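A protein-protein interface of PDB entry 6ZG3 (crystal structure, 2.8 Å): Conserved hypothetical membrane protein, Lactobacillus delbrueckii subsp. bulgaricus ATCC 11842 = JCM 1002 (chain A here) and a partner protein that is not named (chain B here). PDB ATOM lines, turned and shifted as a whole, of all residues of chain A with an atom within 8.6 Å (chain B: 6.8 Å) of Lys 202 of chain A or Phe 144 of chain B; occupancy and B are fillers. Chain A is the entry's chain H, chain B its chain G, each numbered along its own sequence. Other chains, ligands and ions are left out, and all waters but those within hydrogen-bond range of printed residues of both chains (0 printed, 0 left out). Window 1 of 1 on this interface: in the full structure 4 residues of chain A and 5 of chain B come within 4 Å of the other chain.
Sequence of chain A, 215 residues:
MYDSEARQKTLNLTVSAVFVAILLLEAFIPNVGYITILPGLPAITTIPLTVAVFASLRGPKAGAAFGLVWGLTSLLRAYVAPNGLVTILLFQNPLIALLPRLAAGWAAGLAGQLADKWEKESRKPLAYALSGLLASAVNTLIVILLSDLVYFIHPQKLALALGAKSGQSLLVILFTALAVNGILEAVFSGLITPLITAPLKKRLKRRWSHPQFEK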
ATOM      1  N   LEU A  57       8.464  -4.337  18.034  1.00  0.00           N
ATOM      2  CA  LEU A  57       9.268  -3.147  18.310  1.00  0.00           C
ATOM      3  C   LEU A  57      10.533  -3.114  17.465  1.00  0.00           C
ATOM      4  O   LEU A  57      10.797  -2.124  16.770  1.00  0.00           O
ATOM      5  CB  LEU A  57       9.658  -3.082  19.793  1.00  0.00           C
ATOM      6  CG  LEU A  57       8.791  -2.568  20.945  1.00  0.00           C
ATOM      7  CD1 LEU A  57       9.700  -2.012  22.082  1.00  0.00           C
ATOM      8  CD2 LEU A  57       7.705  -1.564  20.481  1.00  0.00           C
ATOM      9  N   GLU A 121      -3.310   4.155  10.630  1.00  0.00           N
ATOM     10  CA  GLU A 121      -3.002   3.854  12.024  1.00  0.00           C
ATOM     11  C   GLU A 121      -3.844   2.705  12.566  1.00  0.00           C
ATOM     12  O   GLU A 121      -3.351   1.903  13.361  1.00  0.00           O
ATOM     13  CB  GLU A 121      -3.197   5.110  12.877  1.00  0.00           C
ATOM     14  CG  GLU A 121      -2.067   6.138  12.781  1.00  0.00           C
ATOM     15  CD  GLU A 121      -0.758   5.645  13.380  1.00  0.00           C
ATOM     16  OE1 GLU A 121      -0.799   5.032  14.470  1.00  0.00           O
ATOM     17  OE2 GLU A 121       0.308   5.860  12.757  1.00  0.00           O
ATOM     18  N   TYR A 128      -0.157  -6.222  14.531  1.00  0.00           N
ATOM     19  CA  TYR A 128       0.373  -6.582  15.850  1.00  0.00           C
ATOM     20  C   TYR A 128      -0.324  -7.838  16.388  1.00  0.00           C
ATOM     21  O   TYR A 128       0.317  -8.708  16.997  1.00  0.00           O
ATOM     22  CB  TYR A 128       0.225  -5.418  16.833  1.00  0.00           C
ATOM     23  CG  TYR A 128       0.950  -4.136  16.457  1.00  0.00           C
ATOM     24  CD1 TYR A 128       2.148  -4.145  15.734  1.00  0.00           C
ATOM     25  CD2 TYR A 128       0.415  -2.898  16.824  1.00  0.00           C
ATOM     26  CE1 TYR A 128       2.791  -2.935  15.402  1.00  0.00           C
ATOM     27  CE2 TYR A 128       1.037  -1.706  16.489  1.00  0.00           C
ATOM     28  CZ  TYR A 128       2.218  -1.727  15.778  1.00  0.00           C
ATOM     29  OH  TYR A 128       2.807  -0.522  15.464  1.00  0.00           O
ATOM     30  N   LEU A 195      -2.670  -4.016  22.229  1.00  0.00           N
ATOM     31  CA  LEU A 195      -2.823  -3.187  23.421  1.00  0.00           C
ATOM     32  C   LEU A 195      -1.494  -2.736  24.031  1.00  0.00           C
ATOM     33  O   LEU A 195      -1.454  -1.753  24.777  1.00  0.00           O
ATOM     34  CB  LEU A 195      -3.662  -3.919  24.474  1.00  0.00           C
ATOM     35  CG  LEU A 195      -5.177  -4.057  24.304  1.00  0.00           C
ATOM     36  CD1 LEU A 195      -5.609  -3.995  22.851  1.00  0.00           C
ATOM     37  CD2 LEU A 195      -5.678  -5.315  25.005  1.00  0.00           C
ATOM     38  N   ILE A 196      -0.415  -3.470  23.811  1.00  0.00           N
ATOM     39  CA  ILE A 196       0.884  -3.078  24.328  1.00  0.00           C
ATOM     40  C   ILE A 196       1.717  -2.383  23.264  1.00  0.00           C
ATOM     41  O   ILE A 196       2.423  -1.418  23.541  1.00  0.00           O
ATOM     42  CB  ILE A 196       1.606  -4.297  24.917  1.00  0.00           C
ATOM     43  CG1 ILE A 196       0.995  -4.643  26.272  1.00  0.00           C
ATOM     44  CG2 ILE A 196       3.015  -3.984  25.110  1.00  0.00           C
ATOM     45  CD1 ILE A 196       1.396  -6.004  26.812  1.00  0.00           C
ATOM     46  N   THR A 197       1.643  -2.858  22.040  1.00  0.00           N
ATOM     47  CA  THR A 197       2.487  -2.310  20.999  1.00  0.00           C
ATOM     48  C   THR A 197       2.118  -0.867  20.655  1.00  0.00           C
ATOM     49  O   THR A 197       3.013  -0.048  20.406  1.00  0.00           O
ATOM     50  CB  THR A 197       2.402  -3.217  19.780  1.00  0.00           C
ATOM     51  OG1 THR A 197       2.648  -4.561  20.203  1.00  0.00           O
ATOM     52  CG2 THR A 197       3.428  -2.837  18.738  1.00  0.00           C
ATOM     53  N   ALA A 198       0.808  -0.523  20.620  1.00  0.00           N
ATOM     54  CA  ALA A 198       0.440   0.838  20.209  1.00  0.00           C
ATOM     55  C   ALA A 198       0.746   1.882  21.283  1.00  0.00           C
ATOM     56  O   ALA A 198       1.364   2.917  20.955  1.00  0.00           O
ATOM     57  CB  ALA A 198      -1.019   0.885  19.751  1.00  0.00           C
ATOM     58  N   PRO A 199       0.369   1.697  22.551  1.00  0.00           N
ATOM     59  CA  PRO A 199       0.880   2.613  23.571  1.00  0.00           C
ATOM     60  C   PRO A 199       2.374   2.810  23.462  1.00  0.00           C
ATOM     61  O   PRO A 199       2.811   3.959  23.540  1.00  0.00           O
ATOM     62  CB  PRO A 199       0.505   1.915  24.875  1.00  0.00           C
ATOM     63  CG  PRO A 199      -0.730   1.226  24.534  1.00  0.00           C
ATOM     64  CD  PRO A 199      -0.521   0.689  23.142  1.00  0.00           C
ATOM     65  N   LEU A 200       3.164   1.755  23.232  1.00  0.00           N
ATOM     66  CA  LEU A 200       4.612   1.928  23.103  1.00  0.00           C
ATOM     67  C   LEU A 200       4.986   2.824  21.936  1.00  0.00           C
ATOM     68  O   LEU A 200       5.933   3.608  22.040  1.00  0.00           O
ATOM     69  CB  LEU A 200       5.335   0.595  23.009  1.00  0.00           C
ATOM     70  CG  LEU A 200       5.788   0.085  24.366  1.00  0.00           C
ATOM     71  CD1 LEU A 200       4.657  -0.159  25.345  1.00  0.00           C
ATOM     72  CD2 LEU A 200       6.625  -1.143  24.201  1.00  0.00           C
ATOM     73  N   LYS A 201       4.323   2.686  20.795  1.00  0.00           N
ATOM     74  CA  LYS A 201       4.582   3.651  19.730  1.00  0.00           C
ATOM     75  C   LYS A 201       4.297   5.068  20.206  1.00  0.00           C
ATOM     76  O   LYS A 201       5.051   6.004  19.900  1.00  0.00           O
ATOM     77  CB  LYS A 201       3.752   3.320  18.501  1.00  0.00           C
ATOM     78  CG  LYS A 201       4.192   2.037  17.842  1.00  0.00           C
ATOM     79  CD  LYS A 201       5.574   2.180  17.229  1.00  0.00           C
ATOM     80  CE  LYS A 201       6.118   0.809  16.853  1.00  0.00           C
ATOM     81  NZ  LYS A 201       6.134  -0.129  18.044  1.00  0.00           N
ATOM     82  N   LYS A 202       3.198   5.243  20.949  1.00  0.00           N
ATOM     83  CA  LYS A 202       2.861   6.563  21.477  1.00  0.00           C
ATOM     84  C   LYS A 202       3.964   7.101  22.391  1.00  0.00           C
ATOM     85  O   LYS A 202       4.530   8.167  22.133  1.00  0.00           O
ATOM     86  CB  LYS A 202       1.506   6.506  22.195  1.00  0.00           C
ATOM     87  CG  LYS A 202       0.417   6.005  21.263  1.00  0.00           C
ATOM     88  CD  LYS A 202      -0.747   6.938  21.216  1.00  0.00           C
ATOM     89  CE  LYS A 202      -1.484   6.870  19.892  1.00  0.00           C
ATOM     90  NZ  LYS A 202      -0.918   7.824  18.883  1.00  0.00           N
ATOM     91  N   ARG A 203       4.326   6.346  23.429  1.00  0.00           N
ATOM     92  CA  ARG A 203       5.343   6.788  24.369  1.00  0.00           C
ATOM     93  C   ARG A 203       6.709   6.960  23.710  1.00  0.00           C
ATOM     94  O   ARG A 203       7.636   7.468  24.351  1.00  0.00           O
ATOM     95  CB  ARG A 203       5.425   5.781  25.511  1.00  0.00           C
ATOM     96  CG  ARG A 203       5.045   6.326  26.848  1.00  0.00           C
ATOM     97  CD  ARG A 203       4.900   7.809  26.811  1.00  0.00           C
ATOM     98  NE  ARG A 203       5.115   8.297  28.158  1.00  0.00           N
ATOM     99  CZ  ARG A 203       5.147   9.578  28.481  1.00  0.00           C
ATOM    100  NH1 ARG A 203       5.367   9.943  29.746  1.00  0.00           N
ATOM    101  NH2 ARG A 203       4.958  10.490  27.534  1.00  0.00           N
ATOM    102  N   LEU A 204       6.851   6.546  22.451  1.00  0.00           N
ATOM    103  CA  LEU A 204       8.092   6.615  21.702  1.00  0.00           C
ATOM    104  C   LEU A 204       8.004   7.630  20.572  1.00  0.00           C
ATOM    105  O   LEU A 204       8.700   7.497  19.565  1.00  0.00           O
ATOM    106  CB  LEU A 204       8.437   5.221  21.188  1.00  0.00           C
ATOM    107  CG  LEU A 204       9.859   4.790  20.802  1.00  0.00           C
ATOM    108  CD1 LEU A 204      10.052   3.332  21.224  1.00  0.00           C
ATOM    109  CD2 LEU A 204      10.142   4.926  19.297  1.00  0.00           C
ATOM    110  N   LYS A 205       7.127   8.634  20.709  1.00  0.00           N
ATOM    111  CA  LYS A 205       6.928   9.605  19.628  1.00  0.00           C
ATOM    112  C   LYS A 205       8.236  10.301  19.234  1.00  0.00           C
ATOM    113  O   LYS A 205       8.489  10.520  18.041  1.00  0.00           O
ATOM    114  CB  LYS A 205       5.869  10.649  19.996  1.00  0.00           C
ATOM    115  CG  LYS A 205       6.088  11.465  21.280  1.00  0.00           C
ATOM    116  CD  LYS A 205       5.761  10.798  22.605  1.00  0.00           C
ATOM    117  CE  LYS A 205       4.954  11.737  23.492  1.00  0.00           C
ATOM    118  NZ  LYS A 205       5.176  11.485  24.931  1.00  0.00           N
ATOM    119  N   ARG A 206       9.111  10.593  20.209  1.00  0.00           N
ATOM    120  CA  ARG A 206      10.374  11.296  19.970  1.00  0.00           C
ATOM    121  C   ARG A 206      11.560  10.337  19.841  1.00  0.00           C
ATOM    122  O   ARG A 206      11.667   9.351  20.580  1.00  0.00           O
ATOM    123  CB  ARG A 206      10.668  12.293  21.098  1.00  0.00           C
ATOM    124  CG  ARG A 206       9.444  12.909  21.737  1.00  0.00           C
ATOM    125  CD  ARG A 206       8.994  12.141  22.978  1.00  0.00           C
ATOM    126  NE  ARG A 206       9.317  12.844  24.218  1.00  0.00           N
ATOM    127  CZ  ARG A 206       8.725  13.965  24.638  1.00  0.00           C
ATOM    128  NH1 ARG A 206       7.769  14.547  23.915  1.00  0.00           N
ATOM    129  NH2 ARG A 206       9.102  14.516  25.788  1.00  0.00           N
ATOM    130  N   GLU B  95       0.586   8.486  37.274  1.00  0.00           N
ATOM    131  CA  GLU B  95       0.496   8.400  35.821  1.00  0.00           C
ATOM    132  C   GLU B  95       0.892   7.020  35.308  1.00  0.00           C
ATOM    133  O   GLU B  95       0.589   6.702  34.150  1.00  0.00           O
ATOM    134  CB  GLU B  95       1.381   9.461  35.166  1.00  0.00           C
ATOM    135  CG  GLU B  95       2.795   9.517  35.779  1.00  0.00           C
ATOM    136  CD  GLU B  95       2.877  10.403  37.035  1.00  0.00           C
ATOM    137  OE1 GLU B  95       1.908  10.400  37.841  1.00  0.00           O
ATOM    138  OE2 GLU B  95       3.920  11.072  37.235  1.00  0.00           O
ATOM    139  N   ALA B  96       1.534   6.196  36.150  1.00  0.00           N
ATOM    140  CA  ALA B  96       1.895   4.826  35.797  1.00  0.00           C
ATOM    141  C   ALA B  96       0.681   3.909  35.666  1.00  0.00           C
ATOM    142  O   ALA B  96       0.749   2.903  34.948  1.00  0.00           O
ATOM    143  CB  ALA B  96       2.873   4.284  36.839  1.00  0.00           C
ATOM    144  N   GLN B  97      -0.429   4.265  36.321  1.00  0.00           N
ATOM    145  CA  GLN B  97      -1.689   3.521  36.240  1.00  0.00           C
ATOM    146  C   GLN B  97      -2.299   3.554  34.836  1.00  0.00           C
ATOM    147  O   GLN B  97      -2.924   2.574  34.405  1.00  0.00           O
ATOM    148  CB  GLN B  97      -2.700   4.124  37.231  1.00  0.00           C
ATOM    149  CG  GLN B  97      -2.198   4.356  38.657  1.00  0.00           C
ATOM    150  CD  GLN B  97      -3.306   4.790  39.578  1.00  0.00           C
ATOM    151  OE1 GLN B  97      -4.481   4.750  39.202  1.00  0.00           O
ATOM    152  NE2 GLN B  97      -2.950   5.208  40.787  1.00  0.00           N
ATOM    153  N   LEU B  98      -2.158   4.681  34.137  1.00  0.00           N
ATOM    154  CA  LEU B  98      -2.781   4.896  32.842  1.00  0.00           C
ATOM    155  C   LEU B  98      -2.472   3.756  31.872  1.00  0.00           C
ATOM    156  O   LEU B  98      -1.324   3.317  31.750  1.00  0.00           O
ATOM    157  CB  LEU B  98      -2.288   6.225  32.266  1.00  0.00           C
ATOM    158  CG  LEU B  98      -2.938   7.525  32.736  1.00  0.00           C
ATOM    159  CD1 LEU B  98      -2.955   7.558  34.223  1.00  0.00           C
ATOM    160  CD2 LEU B  98      -2.230   8.763  32.197  1.00  0.00           C
ATOM    161  N   PHE B  99      -3.514   3.270  31.175  1.00  0.00           N
ATOM    162  CA  PHE B  99      -3.353   2.141  30.257  1.00  0.00           C
ATOM    163  C   PHE B  99      -4.396   2.034  29.135  1.00  0.00           C
ATOM    164  O   PHE B  99      -4.268   1.167  28.269  1.00  0.00           O
ATOM    165  CB  PHE B  99      -3.375   0.829  31.056  1.00  0.00           C
ATOM    166  CG  PHE B  99      -4.752   0.453  31.540  1.00  0.00           C
ATOM    167  CD1 PHE B  99      -5.297   1.046  32.680  1.00  0.00           C
ATOM    168  CD2 PHE B  99      -5.524  -0.458  30.835  1.00  0.00           C
ATOM    169  CE1 PHE B  99      -6.578   0.714  33.112  1.00  0.00           C
ATOM    170  CE2 PHE B  99      -6.795  -0.778  31.264  1.00  0.00           C
ATOM    171  CZ  PHE B  99      -7.317  -0.195  32.397  1.00  0.00           C
ATOM    172  N   GLU B 100      -5.396   2.899  29.080  1.00  0.00           N
ATOM    173  CA  GLU B 100      -6.449   2.642  28.103  1.00  0.00           C
ATOM    174  C   GLU B 100      -6.195   3.352  26.777  1.00  0.00           C
ATOM    175  O   GLU B 100      -5.335   4.220  26.658  1.00  0.00           O
ATOM    176  CB  GLU B 100      -7.810   3.031  28.659  1.00  0.00           C
ATOM    177  CG  GLU B 100      -8.276   2.066  29.739  1.00  0.00           C
ATOM    178  CD  GLU B 100      -9.166   0.960  29.196  1.00  0.00           C
ATOM    179  OE1 GLU B 100      -9.042   0.626  27.995  1.00  0.00           O
ATOM    180  OE2 GLU B 100      -9.987   0.428  29.975  1.00  0.00           O
ATOM    181  N   ASN B 101      -6.959   2.961  25.765  1.00  0.00           N
ATOM    182  CA  ASN B 101      -6.697   3.451  24.415  1.00  0.00           C
ATOM    183  C   ASN B 101      -7.023   4.915  24.280  1.00  0.00           C
ATOM    184  O   ASN B 101      -6.426   5.609  23.454  1.00  0.00           O
ATOM    185  CB  ASN B 101      -7.506   2.656  23.390  1.00  0.00           C
ATOM    186  CG  ASN B 101      -8.604   1.812  24.031  1.00  0.00           C
ATOM    187  OD1 ASN B 101      -8.393   1.154  25.053  1.00  0.00           O
ATOM    188  ND2 ASN B 101      -9.782   1.828  23.426  1.00  0.00           N
ATOM    189  N   VAL B 103      -7.816   8.494  26.776  1.00  0.00           N
ATOM    190  CA  VAL B 103      -7.810   9.084  28.111  1.00  0.00           C
ATOM    191  C   VAL B 103      -9.133   8.770  28.804  1.00  0.00           C
ATOM    192  O   VAL B 103      -9.171   8.180  29.900  1.00  0.00           O
ATOM    193  CB  VAL B 103      -7.570  10.604  28.005  1.00  0.00           C
ATOM    194  CG1 VAL B 103      -7.913  11.292  29.295  1.00  0.00           C
ATOM    195  CG2 VAL B 103      -6.137  10.881  27.612  1.00  0.00           C
ATOM    196  N   HIS B 141      -7.378  11.386  23.155  1.00  0.00           N
ATOM    197  CA  HIS B 141      -6.022  10.928  22.914  1.00  0.00           C
ATOM    198  C   HIS B 141      -5.722   9.698  23.760  1.00  0.00           C
ATOM    199  O   HIS B 141      -6.462   9.331  24.678  1.00  0.00           O
ATOM    200  CB  HIS B 141      -4.986  12.009  23.234  1.00  0.00           C
ATOM    201  CG  HIS B 141      -4.867  13.082  22.194  1.00  0.00           C
ATOM    202  ND1 HIS B 141      -3.952  14.108  22.293  1.00  0.00           N
ATOM    203  CD2 HIS B 141      -5.550  13.298  21.041  1.00  0.00           C
ATOM    204  CE1 HIS B 141      -4.077  14.913  21.251  1.00  0.00           C
ATOM    205  NE2 HIS B 141      -5.036  14.444  20.475  1.00  0.00           N
ATOM    206  N   SER B 142      -4.620   9.049  23.406  1.00  0.00           N
ATOM    207  CA  SER B 142      -3.999   8.088  24.289  1.00  0.00           C
ATOM    208  C   SER B 142      -3.392   8.813  25.482  1.00  0.00           C
ATOM    209  O   SER B 142      -2.779   9.871  25.323  1.00  0.00           O
ATOM    210  CB  SER B 142      -2.909   7.320  23.554  1.00  0.00           C
ATOM    211  OG  SER B 142      -2.315   6.314  24.357  1.00  0.00           O
ATOM    212  N   PRO B 143      -3.543   8.272  26.683  1.00  0.00           N
ATOM    213  CA  PRO B 143      -2.835   8.845  27.835  1.00  0.00           C
ATOM    214  C   PRO B 143      -1.322   8.933  27.632  1.00  0.00           C
ATOM    215  O   PRO B 143      -0.653   9.714  28.323  1.00  0.00           O
ATOM    216  CB  PRO B 143      -3.182   7.875  28.970  1.00  0.00           C
ATOM    217  CG  PRO B 143      -4.347   7.077  28.466  1.00  0.00           C
ATOM    218  CD  PRO B 143      -4.227   7.016  26.998  1.00  0.00           C
ATOM    219  N   PHE B 144      -0.768   8.180  26.686  1.00  0.00           N
ATOM    220  CA  PHE B 144       0.660   8.148  26.431  1.00  0.00           C
ATOM    221  C   PHE B 144       1.099   9.198  25.425  1.00  0.00           C
ATOM    222  O   PHE B 144       2.304   9.419  25.265  1.00  0.00           O
ATOM    223  CB  PHE B 144       1.033   6.726  26.009  1.00  0.00           C
ATOM    224  CG  PHE B 144       0.530   5.704  26.984  1.00  0.00           C
ATOM    225  CD1 PHE B 144       1.005   5.670  28.272  1.00  0.00           C
ATOM    226  CD2 PHE B 144      -0.507   4.860  26.656  1.00  0.00           C
ATOM    227  CE1 PHE B 144       0.502   4.768  29.185  1.00  0.00           C
ATOM    228  CE2 PHE B 144      -1.017   3.959  27.582  1.00  0.00           C
ATOM    229  CZ  PHE B 144      -0.511   3.916  28.835  1.00  0.00           C
ATOM    230  N   ASP B 145       0.157   9.875  24.771  1.00  0.00           N
ATOM    231  CA  ASP B 145       0.491  11.071  24.004  1.00  0.00           C
ATOM    232  C   ASP B 145       0.707  12.305  24.870  1.00  0.00           C
ATOM    233  O   ASP B 145       1.227  13.308  24.373  1.00  0.00           O
ATOM    234  CB  ASP B 145      -0.614  11.405  23.001  1.00  0.00           C
ATOM    235  CG  ASP B 145      -0.335  10.872  21.608  1.00  0.00           C
ATOM    236  OD1 ASP B 145       0.854  10.806  21.193  1.00  0.00           O
ATOM    237  OD2 ASP B 145      -1.330  10.561  20.914  1.00  0.00           O
ATOM    238  N   LEU B 146       0.315  12.268  26.137  1.00  0.00           N
ATOM    239  CA  LEU B 146       0.331  13.471  26.958  1.00  0.00           C
ATOM    240  C   LEU B 146       1.608  13.608  27.772  1.00  0.00           C
ATOM    241  O   LEU B 146       2.354  12.650  28.003  1.00  0.00           O
ATOM    242  CB  LEU B 146      -0.872  13.553  27.901  1.00  0.00           C
ATOM    243  CG  LEU B 146      -2.287  13.733  27.368  1.00  0.00           C
ATOM    244  CD1 LEU B 146      -2.511  13.213  25.951  1.00  0.00           C
ATOM    245  CD2 LEU B 146      -3.247  13.097  28.352  1.00  0.00           C
ATOM    246  N   SER B 147       1.822  14.844  28.217  1.00  0.00           N
ATOM    247  CA  SER B 147       2.917  15.249  29.073  1.00  0.00           C
ATOM    248  C   SER B 147       2.725  14.709  30.489  1.00  0.00           C
ATOM    249  O   SER B 147       1.658  14.219  30.864  1.00  0.00           O
ATOM    250  CB  SER B 147       2.996  16.770  29.099  1.00  0.00           C
ATOM    251  OG  SER B 147       2.003  17.281  29.982  1.00  0.00           O
ATOM    252  N   MET B 151      -0.642  13.702  32.201  1.00  0.00           N
ATOM    253  CA  MET B 151      -0.788  12.312  32.610  1.00  0.00           C
ATOM    254  C   MET B 151      -1.203  12.227  34.071  1.00  0.00           C
ATOM    255  O   MET B 151      -2.081  11.429  34.426  1.00  0.00           O
ATOM    256  CB  MET B 151       0.510  11.533  32.383  1.00  0.00           C
ATOM    257  CG  MET B 151       0.865  11.325  30.931  1.00  0.00           C
ATOM    258  SD  MET B 151       2.164  10.100  30.773  1.00  0.00           S
ATOM    259  CE  MET B 151       1.251   8.656  31.289  1.00  0.00           C
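The side-chain sulfur (SD) of Met 151 of chain B is in hydrogen-bond range of the guanidinium group (NH1) of Arg 203 of chain A (3.4 Å). The side-chain carboxylate of Asp 145 of chain B is in salt-bridge range of the side-chain amino group of Lys 202 of chain A (3.4 Å). O of Leu 146 of chain B sits at hydrogen-bond distance from NH2 of Arg 203 of chain A (3.4 Å).
The backbone NH (N) of Phe 144 of chain B lies close to the side-chain hydroxyl (OG) of Ser 142 of chain B (3.4 Å).
CD2 of Phe 144 of chain B touches CB of Pro 199 of chain A (3.6 Å). Ser 142 of chain B touches Lys 202 of chain A (CB to CD, 3.2 Å). CB of Phe 144 of chain B touches CB of Lys 202 of chain A, 3.8 Å away. Arg 203 of chain A touches Phe 144 of chain B (CD to O, 3.4 Å). Phe 144 of chain B touches Lys 205 of chain A (O to NZ, 3.6 Å).
Glu 121 of chain A touches none of the printed residues of chain B. Printed residues of chain B within 4 Å of Pro 199 of chain A: Phe 144. Lys 202 of chain A touches just these residues of chain B: Ser 142, Phe 144 and Asp 145. Glu 100 of chain B touches none of the printed residues of chain A. Printed residues of chain A within 4 Å of Ser 142 of chain B: Lys 202. No residue of chain A comes within 4 Å of Pro 143 of chain B. Asp 145 of chain B touches one residue of chain A. Printed residues of chain A within 4 Å of Leu 146 of chain B: Arg 203 (3.4 Å). The nearest printed residue of chain B that does not touch Lys 202 of chain A is Asn 101 of chain B (6.2 Å). The nearest residue of chain A that does not touch Phe 144 of chain B is Leu 200 of chain A (5.9 Å). The nearest printed residue of chain B that does not touch Lys 205 of chain A is Asp 145 of chain B (4.1 Å).
Of the 16 printed residues of chain B, 5 touch a printed residue of chain A. Hydrophobic or aromatic side chains of chain B within 4 Å of the printed part of chain A: Phe 144 and Met 151. Of the 15 printed residues of chain A, 4 touch a printed residue of chain B. Hydrophobic or aromatic side chains of chain A that line the printed part of chain B: Pro 199. Along chain A the printed residues that touch a printed residue of chain B span positions 199 to 205. Among the printed residues, Asp or Glu carboxylates within 4 Å of a Lys or Arg side-chain nitrogen of the other chain: Lys 202 of chain A with Asp 145 of chain B.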
